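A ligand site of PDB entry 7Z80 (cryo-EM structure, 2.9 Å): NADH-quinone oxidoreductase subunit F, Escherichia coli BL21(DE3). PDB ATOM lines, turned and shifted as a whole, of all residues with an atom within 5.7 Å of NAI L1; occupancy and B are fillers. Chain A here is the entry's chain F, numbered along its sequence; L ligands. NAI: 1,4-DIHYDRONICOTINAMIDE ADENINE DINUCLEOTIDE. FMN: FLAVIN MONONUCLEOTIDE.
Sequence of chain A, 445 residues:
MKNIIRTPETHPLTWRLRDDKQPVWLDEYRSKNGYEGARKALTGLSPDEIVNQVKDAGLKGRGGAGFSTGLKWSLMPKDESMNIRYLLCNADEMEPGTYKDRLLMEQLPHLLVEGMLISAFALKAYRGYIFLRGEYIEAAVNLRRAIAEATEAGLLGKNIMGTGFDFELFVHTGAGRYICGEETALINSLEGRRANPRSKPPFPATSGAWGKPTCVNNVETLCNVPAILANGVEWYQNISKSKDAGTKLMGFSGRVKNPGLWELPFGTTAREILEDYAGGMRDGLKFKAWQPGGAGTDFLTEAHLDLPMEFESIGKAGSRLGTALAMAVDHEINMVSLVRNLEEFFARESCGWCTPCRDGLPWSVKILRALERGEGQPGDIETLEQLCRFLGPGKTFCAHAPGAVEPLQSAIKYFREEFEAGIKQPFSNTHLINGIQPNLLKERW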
ATOM      1  N   ARG A  62      -4.209 -19.449 -30.634  1.00  0.00           N
ATOM      2  CA  ARG A  62      -5.277 -18.593 -31.157  1.00  0.00           C
ATOM      3  C   ARG A  62      -6.077 -17.910 -30.059  1.00  0.00           C
ATOM      4  O   ARG A  62      -7.042 -17.216 -30.362  1.00  0.00           O
ATOM      5  CB  ARG A  62      -6.194 -19.403 -32.060  1.00  0.00           C
ATOM      6  CG  ARG A  62      -5.478 -20.133 -33.173  1.00  0.00           C
ATOM      7  CD  ARG A  62      -5.014 -19.170 -34.243  1.00  0.00           C
ATOM      8  NE  ARG A  62      -4.676 -19.834 -35.487  1.00  0.00           N
ATOM      9  CZ  ARG A  62      -3.437 -19.985 -35.950  1.00  0.00           C
ATOM     10  NH1 ARG A  62      -2.394 -19.522 -35.278  1.00  0.00           N
ATOM     11  NH2 ARG A  62      -3.242 -20.611 -37.097  1.00  0.00           N
ATOM     12  N   GLY A  63      -5.699 -18.113 -28.793  1.00  0.00           N
ATOM     13  CA  GLY A  63      -6.353 -17.406 -27.707  1.00  0.00           C
ATOM     14  C   GLY A  63      -6.121 -15.918 -27.715  1.00  0.00           C
ATOM     15  O   GLY A  63      -6.961 -15.170 -27.213  1.00  0.00           O
ATOM     16  N   GLY A  64      -5.004 -15.468 -28.285  1.00  0.00           N
ATOM     17  CA  GLY A  64      -4.725 -14.058 -28.388  1.00  0.00           C
ATOM     18  C   GLY A  64      -3.268 -13.712 -28.141  1.00  0.00           C
ATOM     19  O   GLY A  64      -2.775 -12.697 -28.649  1.00  0.00           O
ATOM     20  N   ALA A  65      -2.570 -14.545 -27.378  1.00  0.00           N
ATOM     21  CA  ALA A  65      -1.174 -14.274 -27.040  1.00  0.00           C
ATOM     22  C   ALA A  65      -0.202 -14.750 -28.104  1.00  0.00           C
ATOM     23  O   ALA A  65       0.925 -14.252 -28.147  1.00  0.00           O
ATOM     24  CB  ALA A  65      -0.827 -14.921 -25.703  1.00  0.00           C
ATOM     25  N   PHE A  67       1.331 -17.697 -28.487  1.00  0.00           N
ATOM     26  CA  PHE A  67       2.372 -18.628 -28.085  1.00  0.00           C
ATOM     27  C   PHE A  67       2.334 -19.880 -28.951  1.00  0.00           C
ATOM     28  O   PHE A  67       1.281 -20.301 -29.439  1.00  0.00           O
ATOM     29  CB  PHE A  67       2.209 -19.015 -26.611  1.00  0.00           C
ATOM     30  CG  PHE A  67       3.442 -19.624 -26.014  1.00  0.00           C
ATOM     31  CD1 PHE A  67       4.561 -18.861 -25.767  1.00  0.00           C
ATOM     32  CD2 PHE A  67       3.472 -20.978 -25.702  1.00  0.00           C
ATOM     33  CE1 PHE A  67       5.692 -19.419 -25.207  1.00  0.00           C
ATOM     34  CE2 PHE A  67       4.598 -21.545 -25.142  1.00  0.00           C
ATOM     35  CZ  PHE A  67       5.711 -20.767 -24.901  1.00  0.00           C
ATOM     36  N   LYS A  72       4.492 -25.325 -26.266  1.00  0.00           N
ATOM     37  CA  LYS A  72       3.726 -25.524 -25.043  1.00  0.00           C
ATOM     38  C   LYS A  72       3.514 -27.013 -24.760  1.00  0.00           C
ATOM     39  O   LYS A  72       3.582 -27.446 -23.606  1.00  0.00           O
ATOM     40  CB  LYS A  72       2.380 -24.806 -25.155  1.00  0.00           C
ATOM     41  CG  LYS A  72       1.497 -24.966 -23.933  1.00  0.00           C
ATOM     42  CD  LYS A  72       0.106 -24.439 -24.194  1.00  0.00           C
ATOM     43  CE  LYS A  72       0.148 -23.000 -24.665  1.00  0.00           C
ATOM     44  NZ  LYS A  72      -1.221 -22.422 -24.710  1.00  0.00           N
ATOM     45  N   LEU A  75       6.505 -28.947 -23.192  1.00  0.00           N
ATOM     46  CA  LEU A  75       6.945 -28.553 -21.858  1.00  0.00           C
ATOM     47  C   LEU A  75       6.331 -29.399 -20.743  1.00  0.00           C
ATOM     48  O   LEU A  75       6.638 -29.163 -19.572  1.00  0.00           O
ATOM     49  CB  LEU A  75       6.638 -27.076 -21.625  1.00  0.00           C
ATOM     50  CG  LEU A  75       7.696 -26.167 -22.237  1.00  0.00           C
ATOM     51  CD1 LEU A  75       7.312 -24.710 -22.062  1.00  0.00           C
ATOM     52  CD2 LEU A  75       9.057 -26.434 -21.623  1.00  0.00           C
ATOM     53  N   ASP A  92     -14.207 -20.258 -22.991  1.00  0.00           N
ATOM     54  CA  ASP A  92     -14.827 -19.134 -22.297  1.00  0.00           C
ATOM     55  C   ASP A  92     -15.204 -18.035 -23.276  1.00  0.00           C
ATOM     56  O   ASP A  92     -16.387 -17.752 -23.492  1.00  0.00           O
ATOM     57  CB  ASP A  92     -13.901 -18.599 -21.207  1.00  0.00           C
ATOM     58  CG  ASP A  92     -14.657 -18.123 -19.982  1.00  0.00           C
ATOM     59  OD1 ASP A  92     -15.772 -18.622 -19.736  1.00  0.00           O
ATOM     60  OD2 ASP A  92     -14.132 -17.244 -19.268  1.00  0.00           O
ATOM     61  N   GLU A  93     -14.197 -17.429 -23.920  1.00  0.00           N
ATOM     62  CA  GLU A  93     -14.363 -16.376 -24.926  1.00  0.00           C
ATOM     63  C   GLU A  93     -15.211 -15.224 -24.397  1.00  0.00           C
ATOM     64  O   GLU A  93     -16.216 -14.827 -24.997  1.00  0.00           O
ATOM     65  CB  GLU A  93     -14.929 -16.938 -26.221  1.00  0.00           C
ATOM     66  CG  GLU A  93     -14.537 -16.154 -27.460  1.00  0.00           C
ATOM     67  CD  GLU A  93     -15.521 -16.334 -28.597  1.00  0.00           C
ATOM     68  OE1 GLU A  93     -16.662 -16.774 -28.343  1.00  0.00           O
ATOM     69  OE2 GLU A  93     -15.150 -16.032 -29.752  1.00  0.00           O
ATOM     70  N   MET A  94     -14.803 -14.703 -23.249  1.00  0.00           N
ATOM     71  CA  MET A  94     -15.562 -13.686 -22.535  1.00  0.00           C
ATOM     72  C   MET A  94     -15.148 -12.267 -22.911  1.00  0.00           C
ATOM     73  O   MET A  94     -15.678 -11.315 -22.343  1.00  0.00           O
ATOM     74  CB  MET A  94     -15.403 -13.890 -21.027  1.00  0.00           C
ATOM     75  CG  MET A  94     -16.444 -14.773 -20.385  1.00  0.00           C
ATOM     76  SD  MET A  94     -17.682 -13.848 -19.467  1.00  0.00           S
ATOM     77  CE  MET A  94     -18.865 -15.145 -19.119  1.00  0.00           C
ATOM     78  N   GLU A  95     -14.217 -12.121 -23.838  1.00  0.00           N
ATOM     79  CA  GLU A  95     -13.735 -10.797 -24.244  1.00  0.00           C
ATOM     80  C   GLU A  95     -14.766 -10.101 -25.120  1.00  0.00           C
ATOM     81  O   GLU A  95     -15.327 -10.726 -26.023  1.00  0.00           O
ATOM     82  CB  GLU A  95     -12.413 -10.924 -25.000  1.00  0.00           C
ATOM     83  CG  GLU A  95     -11.822  -9.607 -25.483  1.00  0.00           C
ATOM     84  CD  GLU A  95     -10.816  -9.022 -24.518  1.00  0.00           C
ATOM     85  OE1 GLU A  95     -10.916  -9.293 -23.305  1.00  0.00           O
ATOM     86  OE2 GLU A  95      -9.905  -8.305 -24.976  1.00  0.00           O
ATOM     87  N   THR A  98     -15.462 -10.500 -29.248  1.00  0.00           N
ATOM     88  CA  THR A  98     -15.051 -11.841 -29.657  1.00  0.00           C
ATOM     89  C   THR A  98     -16.273 -12.732 -29.760  1.00  0.00           C
ATOM     90  O   THR A  98     -17.022 -12.892 -28.778  1.00  0.00           O
ATOM     91  CB  THR A  98     -14.040 -12.426 -28.671  1.00  0.00           C
ATOM     92  OG1 THR A  98     -14.642 -12.514 -27.369  1.00  0.00           O
ATOM     93  CG2 THR A  98     -12.814 -11.551 -28.594  1.00  0.00           C
ATOM     94  N   LYS A 100     -15.925 -15.771 -32.101  1.00  0.00           N
ATOM     95  CA  LYS A 100     -15.462 -16.784 -33.042  1.00  0.00           C
ATOM     96  C   LYS A 100     -15.614 -18.206 -32.512  1.00  0.00           C
ATOM     97  O   LYS A 100     -15.952 -19.121 -33.285  1.00  0.00           O
ATOM     98  CB  LYS A 100     -14.005 -16.511 -33.426  1.00  0.00           C
ATOM     99  CG  LYS A 100     -13.050 -16.315 -32.265  1.00  0.00           C
ATOM    100  CD  LYS A 100     -11.634 -16.085 -32.758  1.00  0.00           C
ATOM    101  CE  LYS A 100     -10.633 -16.074 -31.620  1.00  0.00           C
ATOM    102  NZ  LYS A 100     -10.615 -17.378 -30.904  1.00  0.00           N
ATOM    103  N   TYR A 178     -15.556 -13.182 -16.257  1.00  0.00           N
ATOM    104  CA  TYR A 178     -14.622 -12.926 -17.356  1.00  0.00           C
ATOM    105  C   TYR A 178     -13.228 -13.462 -17.053  1.00  0.00           C
ATOM    106  O   TYR A 178     -12.532 -13.949 -17.951  1.00  0.00           O
ATOM    107  CB  TYR A 178     -14.573 -11.430 -17.647  1.00  0.00           C
ATOM    108  CG  TYR A 178     -13.415 -10.980 -18.517  1.00  0.00           C
ATOM    109  CD1 TYR A 178     -13.426 -11.207 -19.884  1.00  0.00           C
ATOM    110  CD2 TYR A 178     -12.327 -10.324 -17.978  1.00  0.00           C
ATOM    111  CE1 TYR A 178     -12.382 -10.793 -20.690  1.00  0.00           C
ATOM    112  CE2 TYR A 178     -11.280  -9.911 -18.775  1.00  0.00           C
ATOM    113  CZ  TYR A 178     -11.312 -10.148 -20.124  1.00  0.00           C
ATOM    114  OH  TYR A 178     -10.269  -9.732 -20.907  1.00  0.00           O
ATOM    115  N   GLU A 182      -8.672 -16.767 -18.126  1.00  0.00           N
ATOM    116  CA  GLU A 182      -7.256 -16.906 -17.832  1.00  0.00           C
ATOM    117  C   GLU A 182      -6.961 -18.348 -17.413  1.00  0.00           C
ATOM    118  O   GLU A 182      -7.716 -18.929 -16.640  1.00  0.00           O
ATOM    119  CB  GLU A 182      -6.848 -15.945 -16.711  1.00  0.00           C
ATOM    120  CG  GLU A 182      -5.434 -15.401 -16.833  1.00  0.00           C
ATOM    121  CD  GLU A 182      -4.408 -16.254 -16.119  1.00  0.00           C
ATOM    122  OE1 GLU A 182      -4.804 -17.203 -15.413  1.00  0.00           O
ATOM    123  OE2 GLU A 182      -3.203 -15.975 -16.258  1.00  0.00           O
ATOM    124  N   GLU A 183      -5.865 -18.893 -17.937  1.00  0.00           N
ATOM    125  CA  GLU A 183      -5.654 -20.341 -17.887  1.00  0.00           C
ATOM    126  C   GLU A 183      -5.497 -20.856 -16.454  1.00  0.00           C
ATOM    127  O   GLU A 183      -6.038 -21.916 -16.118  1.00  0.00           O
ATOM    128  CB  GLU A 183      -4.433 -20.740 -18.737  1.00  0.00           C
ATOM    129  CG  GLU A 183      -3.114 -20.199 -18.232  1.00  0.00           C
ATOM    130  CD  GLU A 183      -1.932 -20.981 -18.738  1.00  0.00           C
ATOM    131  OE1 GLU A 183      -0.879 -20.353 -18.930  1.00  0.00           O
ATOM    132  OE2 GLU A 183      -2.067 -22.198 -18.950  1.00  0.00           O
ATOM    133  N   LYS A 200       3.161 -17.709 -12.296  1.00  0.00           N
ATOM    134  CA  LYS A 200       3.957 -18.585 -13.125  1.00  0.00           C
ATOM    135  C   LYS A 200       5.384 -18.052 -13.157  1.00  0.00           C
ATOM    136  O   LYS A 200       5.580 -16.847 -13.396  1.00  0.00           O
ATOM    137  CB  LYS A 200       3.380 -18.685 -14.548  1.00  0.00           C
ATOM    138  CG  LYS A 200       1.995 -19.292 -14.599  1.00  0.00           C
ATOM    139  CD  LYS A 200       1.389 -19.182 -15.992  1.00  0.00           C
ATOM    140  CE  LYS A 200       1.017 -17.750 -16.327  1.00  0.00           C
ATOM    141  NZ  LYS A 200       0.239 -17.662 -17.586  1.00  0.00           N
ATOM    142  N   PHE A 203       4.470 -23.324 -14.321  1.00  0.00           N
ATOM    143  CA  PHE A 203       3.495 -23.287 -15.387  1.00  0.00           C
ATOM    144  C   PHE A 203       2.554 -24.493 -15.289  1.00  0.00           C
ATOM    145  O   PHE A 203       2.905 -25.505 -14.669  1.00  0.00           O
ATOM    146  CB  PHE A 203       4.212 -23.264 -16.735  1.00  0.00           C
ATOM    147  CG  PHE A 203       4.816 -21.930 -17.058  1.00  0.00           C
ATOM    148  CD1 PHE A 203       4.078 -20.966 -17.722  1.00  0.00           C
ATOM    149  CD2 PHE A 203       6.110 -21.635 -16.675  1.00  0.00           C
ATOM    150  CE1 PHE A 203       4.625 -19.735 -18.015  1.00  0.00           C
ATOM    151  CE2 PHE A 203       6.669 -20.400 -16.973  1.00  0.00           C
ATOM    152  CZ  PHE A 203       5.922 -19.453 -17.636  1.00  0.00           C
ATOM    153  N   PRO A 204       1.352 -24.398 -15.862  1.00  0.00           N
ATOM    154  CA  PRO A 204       0.408 -25.525 -15.785  1.00  0.00           C
ATOM    155  C   PRO A 204       0.884 -26.798 -16.473  1.00  0.00           C
ATOM    156  O   PRO A 204       0.348 -27.863 -16.172  1.00  0.00           O
ATOM    157  CB  PRO A 204      -0.847 -24.978 -16.459  1.00  0.00           C
ATOM    158  CG  PRO A 204      -0.779 -23.520 -16.230  1.00  0.00           C
ATOM    159  CD  PRO A 204       0.684 -23.171 -16.333  1.00  0.00           C
ATOM    160  N   VAL A 216      -3.723 -26.188 -21.387  1.00  0.00           N
ATOM    161  CA  VAL A 216      -4.907 -25.387 -21.673  1.00  0.00           C
ATOM    162  C   VAL A 216      -4.718 -24.756 -23.047  1.00  0.00           C
ATOM    163  O   VAL A 216      -3.709 -24.087 -23.301  1.00  0.00           O
ATOM    164  CB  VAL A 216      -5.135 -24.308 -20.612  1.00  0.00           C
ATOM    165  CG1 VAL A 216      -6.438 -23.566 -20.869  1.00  0.00           C
ATOM    166  CG2 VAL A 216      -5.135 -24.925 -19.227  1.00  0.00           C
ATOM    167  N   ASN A 218      -6.919 -22.914 -26.628  1.00  0.00           N
ATOM    168  CA  ASN A 218      -8.128 -22.288 -27.146  1.00  0.00           C
ATOM    169  C   ASN A 218      -8.888 -23.262 -28.049  1.00  0.00           C
ATOM    170  O   ASN A 218      -8.371 -24.297 -28.470  1.00  0.00           O
ATOM    171  CB  ASN A 218      -7.779 -21.012 -27.897  1.00  0.00           C
ATOM    172  CG  ASN A 218      -8.974 -20.083 -28.073  1.00  0.00           C
ATOM    173  OD1 ASN A 218      -9.976 -20.210 -27.365  1.00  0.00           O
ATOM    174  ND2 ASN A 218      -8.881 -19.174 -29.020  1.00  0.00           N
ATOM    175  N   ARG A 320      -1.921  -4.668 -30.367  1.00  0.00           N
ATOM    176  CA  ARG A 320      -1.838  -6.126 -30.288  1.00  0.00           C
ATOM    177  C   ARG A 320      -2.782  -6.716 -31.323  1.00  0.00           C
ATOM    178  O   ARG A 320      -3.825  -6.139 -31.622  1.00  0.00           O
ATOM    179  CB  ARG A 320      -2.204  -6.639 -28.902  1.00  0.00           C
ATOM    180  CG  ARG A 320      -1.164  -6.370 -27.831  1.00  0.00           C
ATOM    181  CD  ARG A 320      -1.312  -7.333 -26.651  1.00  0.00           C
ATOM    182  NE  ARG A 320      -2.529  -7.101 -25.880  1.00  0.00           N
ATOM    183  CZ  ARG A 320      -3.630  -7.829 -25.977  1.00  0.00           C
ATOM    184  NH1 ARG A 320      -3.725  -8.824 -26.850  1.00  0.00           N
ATOM    185  NH2 ARG A 320      -4.665  -7.556 -25.188  1.00  0.00           N
ATOM    186  N   GLY A 322      -4.274  -9.617 -30.810  1.00  0.00           N
ATOM    187  CA  GLY A 322      -5.353 -10.113 -29.980  1.00  0.00           C
ATOM    188  C   GLY A 322      -6.041 -11.317 -30.595  1.00  0.00           C
ATOM    189  O   GLY A 322      -5.396 -12.244 -31.086  1.00  0.00           O
ATOM    190  N   THR A 323      -7.369 -11.280 -30.591  1.00  0.00           N
ATOM    191  CA  THR A 323      -8.183 -12.335 -31.178  1.00  0.00           C
ATOM    192  C   THR A 323      -8.494 -12.081 -32.649  1.00  0.00           C
ATOM    193  O   THR A 323      -9.285 -12.831 -33.236  1.00  0.00           O
ATOM    194  CB  THR A 323      -9.491 -12.486 -30.401  1.00  0.00           C
ATOM    195  OG1 THR A 323     -10.387 -11.449 -30.784  1.00  0.00           O
ATOM    196  CG2 THR A 323      -9.213 -12.380 -28.909  1.00  0.00           C
ATOM    197  N   CYS A 398      -1.826 -10.675 -12.773  1.00  0.00           N
ATOM    198  CA  CYS A 398      -2.118 -11.292 -14.058  1.00  0.00           C
ATOM    199  C   CYS A 398      -2.220 -10.233 -15.144  1.00  0.00           C
ATOM    200  O   CYS A 398      -1.929  -9.062 -14.893  1.00  0.00           O
ATOM    201  CB  CYS A 398      -3.399 -12.136 -13.977  1.00  0.00           C
ATOM    202  SG  CYS A 398      -4.919 -11.255 -14.354  1.00  0.00           S
ATOM    203  N   ALA A 399      -2.634 -10.630 -16.347  1.00  0.00           N
ATOM    204  CA  ALA A 399      -2.619  -9.742 -17.505  1.00  0.00           C
ATOM    205  C   ALA A 399      -3.982  -9.131 -17.809  1.00  0.00           C
ATOM    206  O   ALA A 399      -4.189  -8.619 -18.907  1.00  0.00           O
ATOM    207  CB  ALA A 399      -2.081 -10.488 -18.733  1.00  0.00           C
HETATM  208  PA  NAI L   1       0.874 -15.282 -21.547  1.00  0.00           P
HETATM  209  O1A NAI L   1       1.420 -14.718 -22.804  1.00  0.00           O
HETATM  210  O2A NAI L   1       1.848 -15.299 -20.380  1.00  0.00           O
HETATM  211  O5B NAI L   1       0.393 -16.791 -21.767  1.00  0.00           O
HETATM  212  C5B NAI L   1      -0.296 -17.245 -22.953  1.00  0.00           C
HETATM  213  C4B NAI L   1       0.054 -18.690 -23.210  1.00  0.00           C
HETATM  214  O4B NAI L   1       1.472 -18.813 -23.416  1.00  0.00           O
HETATM  215  C3B NAI L   1      -0.314 -19.653 -22.071  1.00  0.00           C
HETATM  216  O3B NAI L   1      -0.970 -20.819 -22.564  1.00  0.00           O
HETATM  217  C2B NAI L   1       1.040 -19.959 -21.426  1.00  0.00           C
HETATM  218  O2B NAI L   1       1.074 -21.286 -20.883  1.00  0.00           O
HETATM  219  C1B NAI L   1       1.996 -19.845 -22.597  1.00  0.00           C
HETATM  220  N9A NAI L   1       3.349 -19.468 -22.216  1.00  0.00           N
HETATM  221  C8A NAI L   1       3.936 -18.233 -22.329  1.00  0.00           C
HETATM  222  N7A NAI L   1       5.176 -18.191 -21.916  1.00  0.00           N
HETATM  223  C5A NAI L   1       5.423 -19.491 -21.479  1.00  0.00           C
HETATM  224  C6A NAI L   1       6.554 -20.107 -20.927  1.00  0.00           C
HETATM  225  N6A NAI L   1       7.711 -19.478 -20.703  1.00  0.00           N
HETATM  226  N1A NAI L   1       6.464 -21.418 -20.604  1.00  0.00           N
HETATM  227  C2A NAI L   1       5.311 -22.048 -20.819  1.00  0.00           C
HETATM  228  N3A NAI L   1       4.182 -21.580 -21.348  1.00  0.00           N
HETATM  229  C4A NAI L   1       4.296 -20.280 -21.660  1.00  0.00           C
HETATM  230  O3  NAI L   1      -0.409 -14.481 -21.063  1.00  0.00           O
HETATM  231  PN  NAI L   1      -1.886 -14.851 -20.607  1.00  0.00           P
HETATM  232  O1N NAI L   1      -2.217 -13.966 -19.401  1.00  0.00           O
HETATM  233  O2N NAI L   1      -2.088 -16.293 -20.387  1.00  0.00           O
HETATM  234  O5D NAI L   1      -2.791 -14.306 -21.817  1.00  0.00           O
HETATM  235  C5D NAI L   1      -2.817 -12.899 -22.155  1.00  0.00           C
HETATM  236  C4D NAI L   1      -3.407 -12.729 -23.535  1.00  0.00           C
HETATM  237  O4D NAI L   1      -4.710 -13.333 -23.576  1.00  0.00           O
HETATM  238  C3D NAI L   1      -3.645 -11.283 -23.945  1.00  0.00           C
HETATM  239  O3D NAI L   1      -2.467 -10.716 -24.501  1.00  0.00           O
HETATM  240  C2D NAI L   1      -4.775 -11.399 -24.969  1.00  0.00           C
HETATM  241  O2D NAI L   1      -4.272 -11.408 -26.310  1.00  0.00           O
HETATM  242  C1D NAI L   1      -5.449 -12.739 -24.629  1.00  0.00           C
HETATM  243  N1N NAI L   1      -6.843 -12.598 -24.191  1.00  0.00           N
HETATM  244  C2N NAI L   1      -7.854 -13.356 -24.786  1.00  0.00           C
HETATM  245  C3N NAI L   1      -9.143 -13.267 -24.431  1.00  0.00           C
HETATM  246  C7N NAI L   1     -10.116 -14.112 -25.152  1.00  0.00           C
HETATM  247  O7N NAI L   1      -9.770 -14.750 -26.156  1.00  0.00           O
HETATM  248  N7N NAI L   1     -11.367 -14.148 -24.699  1.00  0.00           N
HETATM  249  C4N NAI L   1      -9.563 -12.342 -23.324  1.00  0.00           C
HETATM  250  C5N NAI L   1      -8.418 -11.569 -22.781  1.00  0.00           C
HETATM  251  C6N NAI L   1      -7.176 -11.719 -23.213  1.00  0.00           C
HETATM  252  N1  FMN L   2      -8.001 -17.489 -23.612  1.00  0.00           N
HETATM  253  C2  FMN L   2      -9.094 -18.110 -24.176  1.00  0.00           C
HETATM  254  O2  FMN L   2      -8.922 -19.005 -25.003  1.00  0.00           O
HETATM  255  N3  FMN L   2     -10.369 -17.743 -23.810  1.00  0.00           N
HETATM  256  C4  FMN L   2     -10.542 -16.738 -22.880  1.00  0.00           C
HETATM  257  O4  FMN L   2     -11.674 -16.393 -22.554  1.00  0.00           O
HETATM  258  C4A FMN L   2      -9.448 -16.117 -22.316  1.00  0.00           C
HETATM  259  N5  FMN L   2      -9.625 -15.110 -21.395  1.00  0.00           N
HETATM  260  C5A FMN L   2      -8.536 -14.498 -20.830  1.00  0.00           C
HETATM  261  C6  FMN L   2      -8.745 -13.495 -19.897  1.00  0.00           C
HETATM  262  C7  FMN L   2      -7.663 -12.856 -19.325  1.00  0.00           C
HETATM  263  C7M FMN L   2      -7.906 -11.773 -18.323  1.00  0.00           C
HETATM  264  C8  FMN L   2      -6.368 -13.221 -19.678  1.00  0.00           C
HETATM  265  C8M FMN L   2      -5.193 -12.526 -19.060  1.00  0.00           C
HETATM  266  C9  FMN L   2      -6.158 -14.224 -20.611  1.00  0.00           C
HETATM  267  C9A FMN L   2      -7.249 -14.870 -21.191  1.00  0.00           C
HETATM  268  N10 FMN L   2      -7.069 -15.881 -22.125  1.00  0.00           N
HETATM  269  C10 FMN L   2      -8.170 -16.497 -22.685  1.00  0.00           C
HETATM  270  C1' FMN L   2      -5.695 -16.328 -22.554  1.00  0.00           C
HETATM  271  C2' FMN L   2      -5.226 -17.497 -21.688  1.00  0.00           C
HETATM  272  O2' FMN L   2      -4.383 -17.024 -20.671  1.00  0.00           O
HETATM  273  C3' FMN L   2      -4.487 -18.556 -22.497  1.00  0.00           C
HETATM  274  O3' FMN L   2      -3.800 -17.938 -23.553  1.00  0.00           O
HETATM  275  C4' FMN L   2      -5.445 -19.601 -23.056  1.00  0.00           C
HETATM  276  O4' FMN L   2      -6.028 -20.318 -21.980  1.00  0.00           O
HETATM  277  C5' FMN L   2      -4.742 -20.571 -23.991  1.00  0.00           C
HETATM  278  O5' FMN L   2      -4.077 -19.833 -24.978  1.00  0.00           O
HETATM  279  P   FMN L   2      -3.495 -20.554 -26.297  1.00  0.00           P
HETATM  280  O1P FMN L   2      -4.485 -20.388 -27.416  1.00  0.00           O
HETATM  281  O2P FMN L   2      -2.182 -19.896 -26.657  1.00  0.00           O
HETATM  282  O3P FMN L   2      -3.279 -22.022 -26.034  1.00  0.00           O
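O of Gly 64 is in hydrogen-bond range of O2D of NAI L1. The backbone NH (N) of Arg 62 sits at hydrogen-bond distance from an oxygen (O1P) of FMN L2 (3.4 Å). The side-chain amino group (NZ) of Lys 200 lies within salt-bridge range of an oxygen (O2N) of NAI L1, 3.9 Å away. An oxygen (O3B) of NAI L1 sits at hydrogen-bond distance from the side-chain amino group (NZ) of Lys 72 (2.7 Å). An oxygen (O2D) of NAI L1 sits at hydrogen-bond distance from the guanidinium group (NH1) of Arg 320, at 2.7 Å. NZ of Lys 72 is in salt-bridge range of O3P of FMN L2, 2.5 Å away. OE1 of Glu 183 sits at hydrogen-bond distance from O2B of NAI L1 (2.9 Å). The backbone NH of Gly 63 lies within hydrogen-bond range of an oxygen (O1P) of FMN L2, at 2.9 Å. N of Glu 93 lies within hydrogen-bond range of O4 of FMN L2 (3.1 Å). OD1 of Asn 218 lies close to O2 of FMN L2, at 2.9 Å.
An oxygen (O2') of FMN L2 lies within hydrogen-bond range of an oxygen (O2N) of NAI L1.
The side-chain hydroxyl of Tyr 178 sits at hydrogen-bond distance from the side-chain carboxylate of Glu 95 (2.5 Å). O of Val 216 is in hydrogen-bond range of NZ of Lys 72. The side-chain carboxylate of Glu 93 is in hydrogen-bond range of the backbone NH of Lys 100 (2.5 Å). The side-chain amino group (NZ) of Lys 200 lies within salt-bridge range of the side-chain carboxylate (OE1) of Glu 183 (3.2 Å). The backbone NH of Gly 63 sits close to the side-chain amide nitrogen of Asn 218, 3.4 Å away.
O of Gly 63 lies close to O7N of NAI L1 (3.0 Å). Ala 65 touches NAI L1 (CB to C5B, 3.6 Å). Phe 67 touches NAI L1 (CB to O4B, 3.3 Å). CD1 of Leu 75 touches C2A of NAI L1, 3.6 Å away. CA of Glu 93 touches N7N of NAI L1 (3.7 Å). Met 94 touches NAI L1 (N to N7N, 3.8 Å). OE1 of Glu 95 touches C4N of NAI L1 (3.3 Å). Tyr 178 touches NAI L1 (OH to C5N, 3.2 Å). Glu 182 touches NAI L1 (OE2 to O1N, 3.9 Å). Phe 203 touches NAI L1 (CZ to C6A, 3.4 Å). Thr 323 touches NAI L1. Ala 399 touches NAI L1. Along chain A the residues within 4 Å of NAI L1 span positions 63 to 399.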
